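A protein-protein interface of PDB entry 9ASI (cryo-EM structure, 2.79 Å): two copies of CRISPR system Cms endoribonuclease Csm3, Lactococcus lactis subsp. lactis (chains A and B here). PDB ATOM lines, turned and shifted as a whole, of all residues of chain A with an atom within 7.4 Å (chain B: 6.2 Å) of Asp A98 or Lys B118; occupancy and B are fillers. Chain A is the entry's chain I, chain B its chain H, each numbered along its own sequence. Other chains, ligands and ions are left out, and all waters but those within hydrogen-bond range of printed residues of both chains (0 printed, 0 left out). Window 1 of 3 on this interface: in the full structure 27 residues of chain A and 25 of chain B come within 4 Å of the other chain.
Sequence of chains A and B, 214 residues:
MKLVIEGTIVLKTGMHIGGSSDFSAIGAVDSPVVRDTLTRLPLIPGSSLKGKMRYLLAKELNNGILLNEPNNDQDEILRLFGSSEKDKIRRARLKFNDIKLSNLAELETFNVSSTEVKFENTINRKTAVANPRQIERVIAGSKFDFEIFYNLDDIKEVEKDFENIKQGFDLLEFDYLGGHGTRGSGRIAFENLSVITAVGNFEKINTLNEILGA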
ATOM      1  N   GLY A  18     -31.053 -33.523 -12.948  1.00  0.00           N
ATOM      2  CA  GLY A  18     -31.810 -34.577 -12.312  1.00  0.00           C
ATOM      3  C   GLY A  18     -31.291 -34.919 -10.930  1.00  0.00           C
ATOM      4  O   GLY A  18     -30.350 -34.319 -10.414  1.00  0.00           O
ATOM      5  N   GLY A  19     -31.912 -35.931 -10.336  1.00  0.00           N
ATOM      6  CA  GLY A  19     -31.589 -36.312  -8.978  1.00  0.00           C
ATOM      7  C   GLY A  19     -32.803 -36.409  -8.079  1.00  0.00           C
ATOM      8  O   GLY A  19     -32.682 -36.360  -6.851  1.00  0.00           O
ATOM      9  N   SER A  21     -35.959 -38.466  -6.363  1.00  0.00           N
ATOM     10  CA  SER A  21     -36.138 -39.797  -5.800  1.00  0.00           C
ATOM     11  C   SER A  21     -37.609 -40.063  -5.526  1.00  0.00           C
ATOM     12  O   SER A  21     -37.973 -40.687  -4.525  1.00  0.00           O
ATOM     13  CB  SER A  21     -35.310 -39.969  -4.529  1.00  0.00           C
ATOM     14  OG  SER A  21     -35.410 -41.291  -4.027  1.00  0.00           O
ATOM     15  N   VAL A  34     -33.946 -31.610  -9.933  1.00  0.00           N
ATOM     16  CA  VAL A  34     -33.503 -31.664  -8.546  1.00  0.00           C
ATOM     17  C   VAL A  34     -34.029 -30.433  -7.820  1.00  0.00           C
ATOM     18  O   VAL A  34     -33.896 -29.302  -8.303  1.00  0.00           O
ATOM     19  CB  VAL A  34     -31.970 -31.768  -8.464  1.00  0.00           C
ATOM     20  CG1 VAL A  34     -31.309 -30.589  -9.136  1.00  0.00           C
ATOM     21  CG2 VAL A  34     -31.518 -31.878  -7.025  1.00  0.00           C
ATOM     22  N   LEU A  43     -33.176 -26.486  -7.526  1.00  0.00           N
ATOM     23  CA  LEU A  43     -31.856 -26.420  -6.924  1.00  0.00           C
ATOM     24  C   LEU A  43     -30.801 -26.561  -8.008  1.00  0.00           C
ATOM     25  O   LEU A  43     -30.955 -27.367  -8.930  1.00  0.00           O
ATOM     26  CB  LEU A  43     -31.695 -27.538  -5.886  1.00  0.00           C
ATOM     27  CG  LEU A  43     -30.425 -27.669  -5.049  1.00  0.00           C
ATOM     28  CD1 LEU A  43     -30.232 -26.454  -4.166  1.00  0.00           C
ATOM     29  CD2 LEU A  43     -30.467 -28.939  -4.228  1.00  0.00           C
ATOM     30  N   ILE A  44     -29.740 -25.770  -7.908  1.00  0.00           N
ATOM     31  CA  ILE A  44     -28.525 -26.014  -8.675  1.00  0.00           C
ATOM     32  C   ILE A  44     -27.497 -26.596  -7.708  1.00  0.00           C
ATOM     33  O   ILE A  44     -27.024 -25.886  -6.808  1.00  0.00           O
ATOM     34  CB  ILE A  44     -27.996 -24.746  -9.357  1.00  0.00           C
ATOM     35  CG1 ILE A  44     -28.820 -24.433 -10.603  1.00  0.00           C
ATOM     36  CG2 ILE A  44     -26.541 -24.920  -9.756  1.00  0.00           C
ATOM     37  CD1 ILE A  44     -28.324 -23.242 -11.373  1.00  0.00           C
ATOM     38  N   PRO A  45     -27.147 -27.874  -7.826  1.00  0.00           N
ATOM     39  CA  PRO A  45     -26.172 -28.455  -6.896  1.00  0.00           C
ATOM     40  C   PRO A  45     -24.794 -27.853  -7.123  1.00  0.00           C
ATOM     41  O   PRO A  45     -24.285 -27.839  -8.246  1.00  0.00           O
ATOM     42  CB  PRO A  45     -26.199 -29.953  -7.219  1.00  0.00           C
ATOM     43  CG  PRO A  45     -26.992 -30.112  -8.452  1.00  0.00           C
ATOM     44  CD  PRO A  45     -27.624 -28.827  -8.839  1.00  0.00           C
ATOM     45  N   GLY A  46     -24.193 -27.351  -6.045  1.00  0.00           N
ATOM     46  CA  GLY A  46     -22.863 -26.787  -6.144  1.00  0.00           C
ATOM     47  C   GLY A  46     -21.832 -27.782  -6.614  1.00  0.00           C
ATOM     48  O   GLY A  46     -20.774 -27.379  -7.110  1.00  0.00           O
ATOM     49  N   SER A  47     -22.124 -29.079  -6.485  1.00  0.00           N
ATOM     50  CA  SER A  47     -21.275 -30.100  -7.088  1.00  0.00           C
ATOM     51  C   SER A  47     -21.375 -30.071  -8.604  1.00  0.00           C
ATOM     52  O   SER A  47     -20.366 -30.217  -9.296  1.00  0.00           O
ATOM     53  CB  SER A  47     -21.641 -31.479  -6.548  1.00  0.00           C
ATOM     54  OG  SER A  47     -23.017 -31.749  -6.714  1.00  0.00           O
ATOM     55  N   SER A  48     -22.581 -29.867  -9.142  1.00  0.00           N
ATOM     56  CA  SER A  48     -22.736 -29.761 -10.590  1.00  0.00           C
ATOM     57  C   SER A  48     -22.016 -28.534 -11.132  1.00  0.00           C
ATOM     58  O   SER A  48     -21.302 -28.610 -12.138  1.00  0.00           O
ATOM     59  CB  SER A  48     -24.219 -29.714 -10.955  1.00  0.00           C
ATOM     60  OG  SER A  48     -24.792 -31.010 -10.952  1.00  0.00           O
ATOM     61  N   LYS A  95     -15.140 -23.080  -2.421  1.00  0.00           N
ATOM     62  CA  LYS A  95     -16.157 -23.826  -1.689  1.00  0.00           C
ATOM     63  C   LYS A  95     -17.506 -23.482  -2.313  1.00  0.00           C
ATOM     64  O   LYS A  95     -18.167 -22.524  -1.911  1.00  0.00           O
ATOM     65  CB  LYS A  95     -16.121 -23.495  -0.201  1.00  0.00           C
ATOM     66  CG  LYS A  95     -16.785 -24.525   0.694  1.00  0.00           C
ATOM     67  CD  LYS A  95     -18.265 -24.250   0.852  1.00  0.00           C
ATOM     68  CE  LYS A  95     -18.924 -25.318   1.693  1.00  0.00           C
ATOM     69  NZ  LYS A  95     -20.402 -25.314   1.594  1.00  0.00           N
ATOM     70  N   PHE A  96     -17.906 -24.272  -3.303  1.00  0.00           N
ATOM     71  CA  PHE A  96     -19.206 -24.090  -3.926  1.00  0.00           C
ATOM     72  C   PHE A  96     -20.307 -24.539  -2.976  1.00  0.00           C
ATOM     73  O   PHE A  96     -20.096 -25.378  -2.100  1.00  0.00           O
ATOM     74  CB  PHE A  96     -19.290 -24.873  -5.232  1.00  0.00           C
ATOM     75  CG  PHE A  96     -18.341 -24.395  -6.290  1.00  0.00           C
ATOM     76  CD1 PHE A  96     -17.002 -24.722  -6.236  1.00  0.00           C
ATOM     77  CD2 PHE A  96     -18.794 -23.628  -7.343  1.00  0.00           C
ATOM     78  CE1 PHE A  96     -16.136 -24.294  -7.206  1.00  0.00           C
ATOM     79  CE2 PHE A  96     -17.927 -23.192  -8.316  1.00  0.00           C
ATOM     80  CZ  PHE A  96     -16.597 -23.526  -8.247  1.00  0.00           C
ATOM     81  N   ASN A  97     -21.493 -23.969  -3.155  1.00  0.00           N
ATOM     82  CA  ASN A  97     -22.634 -24.287  -2.312  1.00  0.00           C
ATOM     83  C   ASN A  97     -23.841 -24.589  -3.185  1.00  0.00           C
ATOM     84  O   ASN A  97     -23.983 -24.048  -4.282  1.00  0.00           O
ATOM     85  CB  ASN A  97     -22.960 -23.142  -1.351  1.00  0.00           C
ATOM     86  CG  ASN A  97     -21.886 -22.938  -0.306  1.00  0.00           C
ATOM     87  OD1 ASN A  97     -21.648 -23.807   0.525  1.00  0.00           O
ATOM     88  ND2 ASN A  97     -21.225 -21.789  -0.350  1.00  0.00           N
ATOM     89  N   ASP A  98     -24.703 -25.472  -2.691  1.00  0.00           N
ATOM     90  CA  ASP A  98     -25.924 -25.806  -3.411  1.00  0.00           C
ATOM     91  C   ASP A  98     -26.792 -24.567  -3.564  1.00  0.00           C
ATOM     92  O   ASP A  98     -27.232 -23.977  -2.573  1.00  0.00           O
ATOM     93  CB  ASP A  98     -26.680 -26.910  -2.679  1.00  0.00           C
ATOM     94  CG  ASP A  98     -26.002 -28.253  -2.805  1.00  0.00           C
ATOM     95  OD1 ASP A  98     -25.072 -28.371  -3.626  1.00  0.00           O
ATOM     96  OD2 ASP A  98     -26.396 -29.191  -2.084  1.00  0.00           O
ATOM     97  N   ILE A  99     -27.035 -24.178  -4.807  1.00  0.00           N
ATOM     98  CA  ILE A  99     -27.664 -22.902  -5.116  1.00  0.00           C
ATOM     99  C   ILE A  99     -29.163 -23.122  -5.240  1.00  0.00           C
ATOM    100  O   ILE A  99     -29.611 -23.946  -6.044  1.00  0.00           O
ATOM    101  CB  ILE A  99     -27.093 -22.321  -6.416  1.00  0.00           C
ATOM    102  CG1 ILE A  99     -25.573 -22.266  -6.355  1.00  0.00           C
ATOM    103  CG2 ILE A  99     -27.568 -20.915  -6.585  1.00  0.00           C
ATOM    104  CD1 ILE A  99     -24.945 -21.984  -7.688  1.00  0.00           C
ATOM    105  N   LYS A 100     -29.941 -22.374  -4.469  1.00  0.00           N
ATOM    106  CA  LYS A 100     -31.388 -22.530  -4.455  1.00  0.00           C
ATOM    107  C   LYS A 100     -32.046 -21.427  -5.274  1.00  0.00           C
ATOM    108  O   LYS A 100     -31.480 -20.349  -5.462  1.00  0.00           O
ATOM    109  CB  LYS A 100     -31.923 -22.511  -3.023  1.00  0.00           C
ATOM    110  CG  LYS A 100     -33.308 -23.108  -2.868  1.00  0.00           C
ATOM    111  CD  LYS A 100     -33.595 -23.460  -1.424  1.00  0.00           C
ATOM    112  CE  LYS A 100     -33.705 -22.213  -0.565  1.00  0.00           C
ATOM    113  NZ  LYS A 100     -34.115 -22.528   0.830  1.00  0.00           N
ATOM    114  N   LEU A 101     -33.249 -21.715  -5.767  1.00  0.00           N
ATOM    115  CA  LEU A 101     -33.984 -20.737  -6.556  1.00  0.00           C
ATOM    116  C   LEU A 101     -34.369 -19.541  -5.694  1.00  0.00           C
ATOM    117  O   LEU A 101     -34.751 -19.688  -4.531  1.00  0.00           O
ATOM    118  CB  LEU A 101     -35.233 -21.370  -7.164  1.00  0.00           C
ATOM    119  CG  LEU A 101     -35.958 -20.493  -8.185  1.00  0.00           C
ATOM    120  CD1 LEU A 101     -35.385 -20.720  -9.560  1.00  0.00           C
ATOM    121  CD2 LEU A 101     -37.451 -20.756  -8.171  1.00  0.00           C
ATOM    122  N   ASP A 145     -29.336 -17.213  -6.827  1.00  0.00           N
ATOM    123  CA  ASP A 145     -28.365 -16.383  -6.124  1.00  0.00           C
ATOM    124  C   ASP A 145     -27.398 -17.280  -5.360  1.00  0.00           C
ATOM    125  O   ASP A 145     -27.821 -18.058  -4.499  1.00  0.00           O
ATOM    126  CB  ASP A 145     -29.079 -15.429  -5.170  1.00  0.00           C
ATOM    127  CG  ASP A 145     -29.878 -14.366  -5.896  1.00  0.00           C
ATOM    128  OD1 ASP A 145     -29.496 -13.992  -7.022  1.00  0.00           O
ATOM    129  OD2 ASP A 145     -30.889 -13.898  -5.336  1.00  0.00           O
ATOM    130  N   PHE A 146     -26.105 -17.170  -5.658  1.00  0.00           N
ATOM    131  CA  PHE A 146     -25.120 -18.075  -5.088  1.00  0.00           C
ATOM    132  C   PHE A 146     -24.109 -17.330  -4.230  1.00  0.00           C
ATOM    133  O   PHE A 146     -23.964 -16.108  -4.310  1.00  0.00           O
ATOM    134  CB  PHE A 146     -24.393 -18.873  -6.181  1.00  0.00           C
ATOM    135  CG  PHE A 146     -23.486 -18.055  -7.059  1.00  0.00           C
ATOM    136  CD1 PHE A 146     -22.176 -17.800  -6.689  1.00  0.00           C
ATOM    137  CD2 PHE A 146     -23.933 -17.575  -8.276  1.00  0.00           C
ATOM    138  CE1 PHE A 146     -21.340 -17.066  -7.503  1.00  0.00           C
ATOM    139  CE2 PHE A 146     -23.098 -16.840  -9.094  1.00  0.00           C
ATOM    140  CZ  PHE A 146     -21.801 -16.586  -8.706  1.00  0.00           C
ATOM    141  N   GLU A 147     -23.417 -18.100  -3.388  1.00  0.00           N
ATOM    142  CA  GLU A 147     -22.317 -17.608  -2.562  1.00  0.00           C
ATOM    143  C   GLU A 147     -21.232 -18.674  -2.566  1.00  0.00           C
ATOM    144  O   GLU A 147     -21.411 -19.740  -1.969  1.00  0.00           O
ATOM    145  CB  GLU A 147     -22.772 -17.310  -1.133  1.00  0.00           C
ATOM    146  CG  GLU A 147     -23.886 -16.286  -1.021  1.00  0.00           C
ATOM    147  CD  GLU A 147     -23.853 -15.526   0.292  1.00  0.00           C
ATOM    148  OE1 GLU A 147     -23.387 -16.097   1.300  1.00  0.00           O
ATOM    149  OE2 GLU A 147     -24.292 -14.358   0.316  1.00  0.00           O
ATOM    150  N   LYS B  12     -27.687 -24.923   6.184  1.00  0.00           N
ATOM    151  CA  LYS B  12     -27.995 -24.023   5.082  1.00  0.00           C
ATOM    152  C   LYS B  12     -28.121 -24.787   3.771  1.00  0.00           C
ATOM    153  O   LYS B  12     -29.048 -24.550   2.994  1.00  0.00           O
ATOM    154  CB  LYS B  12     -26.924 -22.936   4.977  1.00  0.00           C
ATOM    155  CG  LYS B  12     -27.034 -21.857   6.040  1.00  0.00           C
ATOM    156  CD  LYS B  12     -28.485 -21.545   6.358  1.00  0.00           C
ATOM    157  CE  LYS B  12     -28.614 -20.266   7.156  1.00  0.00           C
ATOM    158  NZ  LYS B  12     -29.766 -20.326   8.089  1.00  0.00           N
ATOM    159  N   THR B  13     -27.188 -25.690   3.510  1.00  0.00           N
ATOM    160  CA  THR B  13     -27.306 -26.693   2.466  1.00  0.00           C
ATOM    161  C   THR B  13     -27.396 -28.062   3.126  1.00  0.00           C
ATOM    162  O   THR B  13     -27.397 -28.186   4.352  1.00  0.00           O
ATOM    163  CB  THR B  13     -26.125 -26.620   1.493  1.00  0.00           C
ATOM    164  OG1 THR B  13     -24.954 -27.163   2.110  1.00  0.00           O
ATOM    165  CG2 THR B  13     -25.849 -25.184   1.088  1.00  0.00           C
ATOM    166  N   GLY B  14     -27.491 -29.101   2.302  1.00  0.00           N
ATOM    167  CA  GLY B  14     -27.450 -30.447   2.836  1.00  0.00           C
ATOM    168  C   GLY B  14     -26.124 -30.729   3.512  1.00  0.00           C
ATOM    169  O   GLY B  14     -25.069 -30.258   3.086  1.00  0.00           O
ATOM    170  N   GLU B 116     -32.451 -36.505   2.995  1.00  0.00           N
ATOM    171  CA  GLU B 116     -32.717 -36.595   1.570  1.00  0.00           C
ATOM    172  C   GLU B 116     -31.715 -37.542   0.928  1.00  0.00           C
ATOM    173  O   GLU B 116     -30.772 -38.015   1.563  1.00  0.00           O
ATOM    174  CB  GLU B 116     -32.627 -35.217   0.910  1.00  0.00           C
ATOM    175  CG  GLU B 116     -31.193 -34.779   0.654  1.00  0.00           C
ATOM    176  CD  GLU B 116     -31.094 -33.420   0.005  1.00  0.00           C
ATOM    177  OE1 GLU B 116     -31.328 -33.328  -1.217  1.00  0.00           O
ATOM    178  OE2 GLU B 116     -30.769 -32.446   0.713  1.00  0.00           O
ATOM    179  N   VAL B 117     -31.927 -37.811  -0.354  1.00  0.00           N
ATOM    180  CA  VAL B 117     -30.987 -38.575  -1.160  1.00  0.00           C
ATOM    181  C   VAL B 117     -30.482 -37.674  -2.274  1.00  0.00           C
ATOM    182  O   VAL B 117     -31.278 -37.091  -3.018  1.00  0.00           O
ATOM    183  CB  VAL B 117     -31.630 -39.853  -1.725  1.00  0.00           C
ATOM    184  CG1 VAL B 117     -30.813 -40.381  -2.872  1.00  0.00           C
ATOM    185  CG2 VAL B 117     -31.744 -40.902  -0.639  1.00  0.00           C
ATOM    186  N   LYS B 118     -29.163 -37.549  -2.379  1.00  0.00           N
ATOM    187  CA  LYS B 118     -28.525 -36.724  -3.392  1.00  0.00           C
ATOM    188  C   LYS B 118     -27.865 -37.619  -4.430  1.00  0.00           C
ATOM    189  O   LYS B 118     -27.085 -38.510  -4.080  1.00  0.00           O
ATOM    190  CB  LYS B 118     -27.486 -35.786  -2.777  1.00  0.00           C
ATOM    191  CG  LYS B 118     -26.878 -34.840  -3.793  1.00  0.00           C
ATOM    192  CD  LYS B 118     -25.747 -34.025  -3.218  1.00  0.00           C
ATOM    193  CE  LYS B 118     -25.205 -33.064  -4.263  1.00  0.00           C
ATOM    194  NZ  LYS B 118     -24.139 -32.173  -3.732  1.00  0.00           N
ATOM    195  N   PHE B 119     -28.163 -37.367  -5.696  1.00  0.00           N
ATOM    196  CA  PHE B 119     -27.640 -38.160  -6.799  1.00  0.00           C
ATOM    197  C   PHE B 119     -26.500 -37.391  -7.454  1.00  0.00           C
ATOM    198  O   PHE B 119     -26.717 -36.333  -8.050  1.00  0.00           O
ATOM    199  CB  PHE B 119     -28.740 -38.474  -7.805  1.00  0.00           C
ATOM    200  CG  PHE B 119     -29.804 -39.386  -7.275  1.00  0.00           C
ATOM    201  CD1 PHE B 119     -30.902 -38.875  -6.610  1.00  0.00           C
ATOM    202  CD2 PHE B 119     -29.712 -40.753  -7.450  1.00  0.00           C
ATOM    203  CE1 PHE B 119     -31.886 -39.709  -6.126  1.00  0.00           C
ATOM    204  CE2 PHE B 119     -30.697 -41.591  -6.969  1.00  0.00           C
ATOM    205  CZ  PHE B 119     -31.780 -41.069  -6.302  1.00  0.00           C
ATOM    206  N   GLU B 120     -25.294 -37.925  -7.341  1.00  0.00           N
ATOM    207  CA  GLU B 120     -24.105 -37.349  -7.942  1.00  0.00           C
ATOM    208  C   GLU B 120     -23.557 -38.297  -8.999  1.00  0.00           C
ATOM    209  O   GLU B 120     -24.065 -39.402  -9.200  1.00  0.00           O
ATOM    210  CB  GLU B 120     -23.049 -37.059  -6.876  1.00  0.00           C
ATOM    211  CG  GLU B 120     -23.290 -35.809  -6.060  1.00  0.00           C
ATOM    212  CD  GLU B 120     -21.997 -35.177  -5.583  1.00  0.00           C
ATOM    213  OE1 GLU B 120     -20.918 -35.658  -5.983  1.00  0.00           O
ATOM    214  OE2 GLU B 120     -22.058 -34.204  -4.804  1.00  0.00           O
ATOM    215  N   ARG B 133     -23.289 -42.074  -7.886  1.00  0.00           N
ATOM    216  CA  ARG B 133     -23.363 -42.434  -6.482  1.00  0.00           C
ATOM    217  C   ARG B 133     -24.674 -41.911  -5.909  1.00  0.00           C
ATOM    218  O   ARG B 133     -25.492 -41.314  -6.609  1.00  0.00           O
ATOM    219  CB  ARG B 133     -22.163 -41.895  -5.703  1.00  0.00           C
ATOM    220  CG  ARG B 133     -21.901 -40.432  -5.911  1.00  0.00           C
ATOM    221  CD  ARG B 133     -20.540 -40.048  -5.385  1.00  0.00           C
ATOM    222  NE  ARG B 133     -20.168 -38.697  -5.776  1.00  0.00           N
ATOM    223  CZ  ARG B 133     -19.857 -38.333  -7.012  1.00  0.00           C
ATOM    224  NH1 ARG B 133     -19.865 -39.200  -8.008  1.00  0.00           N
ATOM    225  NH2 ARG B 133     -19.537 -37.066  -7.252  1.00  0.00           N
ATOM    226  N   GLN B 134     -24.874 -42.150  -4.620  1.00  0.00           N
ATOM    227  CA  GLN B 134     -26.149 -41.830  -3.990  1.00  0.00           C
ATOM    228  C   GLN B 134     -25.859 -41.470  -2.537  1.00  0.00           C
ATOM    229  O   GLN B 134     -25.759 -42.356  -1.686  1.00  0.00           O
ATOM    230  CB  GLN B 134     -27.101 -43.010  -4.107  1.00  0.00           C
ATOM    231  CG  GLN B 134     -28.550 -42.638  -4.228  1.00  0.00           C
ATOM    232  CD  GLN B 134     -29.359 -43.711  -4.914  1.00  0.00           C
ATOM    233  OE1 GLN B 134     -28.894 -44.345  -5.859  1.00  0.00           O
ATOM    234  NE2 GLN B 134     -30.578 -43.928  -4.436  1.00  0.00           N
ATOM    235  N   ILE B 135     -25.734 -40.176  -2.263  1.00  0.00           N
ATOM    236  CA  ILE B 135     -25.311 -39.690  -0.956  1.00  0.00           C
ATOM    237  C   ILE B 135     -26.557 -39.371  -0.147  1.00  0.00           C
ATOM    238  O   ILE B 135     -27.356 -38.513  -0.537  1.00  0.00           O
ATOM    239  CB  ILE B 135     -24.412 -38.447  -1.068  1.00  0.00           C
ATOM    240  CG1 ILE B 135     -23.123 -38.750  -1.819  1.00  0.00           C
ATOM    241  CG2 ILE B 135     -24.057 -37.923   0.302  1.00  0.00           C
ATOM    242  CD1 ILE B 135     -23.245 -38.553  -3.299  1.00  0.00           C
ATOM    243  N   GLU B 136     -26.737 -40.058   0.974  1.00  0.00           N
ATOM    244  CA  GLU B 136     -27.720 -39.601   1.939  1.00  0.00           C
ATOM    245  C   GLU B 136     -27.241 -38.299   2.559  1.00  0.00           C
ATOM    246  O   GLU B 136     -26.045 -38.094   2.778  1.00  0.00           O
ATOM    247  CB  GLU B 136     -27.954 -40.648   3.022  1.00  0.00           C
ATOM    248  CG  GLU B 136     -29.282 -40.494   3.729  1.00  0.00           C
ATOM    249  CD  GLU B 136     -29.335 -41.265   5.026  1.00  0.00           C
ATOM    250  OE1 GLU B 136     -28.314 -41.883   5.387  1.00  0.00           O
ATOM    251  OE2 GLU B 136     -30.395 -41.253   5.684  1.00  0.00           O
ATOM    252  N   ARG B 137     -28.185 -37.406   2.837  1.00  0.00           N
ATOM    253  CA  ARG B 137     -27.816 -36.066   3.263  1.00  0.00           C
ATOM    254  C   ARG B 137     -28.937 -35.498   4.112  1.00  0.00           C
ATOM    255  O   ARG B 137     -30.110 -35.642   3.765  1.00  0.00           O
ATOM    256  CB  ARG B 137     -27.543 -35.177   2.048  1.00  0.00           C
ATOM    257  CG  ARG B 137     -26.382 -34.227   2.217  1.00  0.00           C
ATOM    258  CD  ARG B 137     -26.039 -33.546   0.910  1.00  0.00           C
ATOM    259  NE  ARG B 137     -27.141 -32.730   0.417  1.00  0.00           N
ATOM    260  CZ  ARG B 137     -27.004 -31.710  -0.418  1.00  0.00           C
ATOM    261  NH1 ARG B 137     -25.816 -31.322  -0.847  1.00  0.00           N
ATOM    262  NH2 ARG B 137     -28.088 -31.064  -0.833  1.00  0.00           N
ATOM    263  N   HIS B 180     -18.815 -33.677   1.884  1.00  0.00           N
ATOM    264  CA  HIS B 180     -18.291 -33.154   0.623  1.00  0.00           C
ATOM    265  C   HIS B 180     -18.571 -31.658   0.505  1.00  0.00           C
ATOM    266  O   HIS B 180     -19.304 -31.196  -0.363  1.00  0.00           O
ATOM    267  CB  HIS B 180     -18.904 -33.924  -0.536  1.00  0.00           C
ATOM    268  CG  HIS B 180     -19.124 -35.371  -0.235  1.00  0.00           C
ATOM    269  ND1 HIS B 180     -18.088 -36.262  -0.059  1.00  0.00           N
ATOM    270  CD2 HIS B 180     -20.262 -36.080  -0.061  1.00  0.00           C
ATOM    271  CE1 HIS B 180     -18.580 -37.459   0.200  1.00  0.00           C
ATOM    272  NE2 HIS B 180     -19.897 -37.376   0.204  1.00  0.00           N
ATOM    273  N   ARG B 183     -18.021 -29.487  -2.705  1.00  0.00           N
ATOM    274  CA  ARG B 183     -19.044 -29.771  -3.712  1.00  0.00           C
ATOM    275  C   ARG B 183     -20.450 -29.486  -3.190  1.00  0.00           C
ATOM    276  O   ARG B 183     -21.336 -30.331  -3.276  1.00  0.00           O
ATOM    277  CB  ARG B 183     -18.926 -31.217  -4.173  1.00  0.00           C
ATOM    278  CG  ARG B 183     -18.200 -31.402  -5.484  1.00  0.00           C
ATOM    279  CD  ARG B 183     -17.597 -32.786  -5.571  1.00  0.00           C
ATOM    280  NE  ARG B 183     -16.530 -32.968  -4.597  1.00  0.00           N
ATOM    281  CZ  ARG B 183     -16.553 -33.871  -3.628  1.00  0.00           C
ATOM    282  NH1 ARG B 183     -17.575 -34.696  -3.477  1.00  0.00           N
ATOM    283  NH2 ARG B 183     -15.525 -33.950  -2.791  1.00  0.00           N
ATOM    284  N   GLY B 184     -20.682 -28.296  -2.637  1.00  0.00           N
ATOM    285  CA  GLY B 184     -22.012 -27.846  -2.297  1.00  0.00           C
ATOM    286  C   GLY B 184     -22.509 -28.187  -0.903  1.00  0.00           C
ATOM    287  O   GLY B 184     -23.294 -27.423  -0.338  1.00  0.00           O
ATOM    288  N   SER B 185     -22.083 -29.311  -0.338  1.00  0.00           N
ATOM    289  CA  SER B 185     -22.665 -29.790   0.906  1.00  0.00           C
ATOM    290  C   SER B 185     -22.066 -29.075   2.114  1.00  0.00           C
ATOM    291  O   SER B 185     -21.112 -28.301   2.011  1.00  0.00           O
ATOM    292  CB  SER B 185     -22.456 -31.297   1.049  1.00  0.00           C
ATOM    293  OG  SER B 185     -23.217 -32.016   0.100  1.00  0.00           O
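Of the printed residues of chain B, Ser A47 touches Lys B118, Glu B120 and Arg B183. Of the printed residues of chain A, Lys B118 touches Ser A47 (3.2 Å) and Asp A98 (3.9 Å). Of the printed residues of chain A, Phe B119 touches Gly A19 (3.1 Å) and Ser A21 (3.8 Å). Of the printed residues of chain A, Arg B137 touches Asp A98 (2.5 Å). Printed residues of chain A within 4 Å of Arg B183: Ser A47 (3.5 Å).
The side-chain amino group of Lys B118 sits at hydrogen-bond distance from the side-chain hydroxyl of Ser A47 (3.2 Å). NZ of Lys B118 is in salt-bridge range of OD1 of Asp A98, 3.9 Å away. The side-chain carboxylate (OE2) of Glu B120 is in hydrogen-bond range of the side-chain hydroxyl (OG) of Ser A47. The guanidinium group of Arg B137 lies within salt-bridge range of the side-chain carboxylate of Asp A98 (2.5 Å). The backbone NH (N) of Gly B184 lies within hydrogen-bond range of the backbone carbonyl oxygen (O) of Phe A96 (3.0 Å). The backbone carbonyl oxygen (O) of Gly B184 lies within hydrogen-bond range of the backbone NH (N) of Asp A98, at 3.4 Å. The backbone carbonyl oxygen of Ser B185 lies within hydrogen-bond range of the side-chain amino group of Lys A95 (3.1 Å).
No position is printed for both chains.
Printed residues of chain A that touch a printed residue of chain B: Gly A19, Ser A21, Ser A47, Lys A95, Phe A96, Asn A97 and Asp A98. Printed residues of chain B that touch a printed residue of chain A: Thr B13, Lys B118, Phe B119, Glu B120, Arg B137, Arg B183, Gly B184 and Ser B185. Hydrophobic or aromatic side chains of chain B within 4 Å of the printed part of chain A: Phe B119.
Among the printed residues, pairs that only touch across the chains: Gly A19 with Phe B119 (3.1 Å), Ser A21 with Phe B119 (3.8 Å), Ser A47 with Arg B183 (3.5 Å), Asn A97 with Gly B184 (3.6 Å) and Asp A98 with Thr B13 (3.96 Å).
OG1 of Thr B13 lies within hydrogen-bond range of O of Gly B184 (3.0 Å). OE2 of Glu B116 is in salt-bridge range of NH2 of Arg B137, at 3.4 Å. The side-chain amino group of Lys B118 is in salt-bridge range of the side-chain carboxylate of Glu B120 (3.1 Å). The side-chain carboxylate (OE1) of Glu B120 is in salt-bridge range of the guanidinium group (NE) of Arg B133 (3.1 Å). NH1 of Arg B137 is in hydrogen-bond range of OG of Ser B185, at 2.9 Å. ND2 of Asn A97 is in hydrogen-bond range of O of Glu A147 (2.6 Å).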
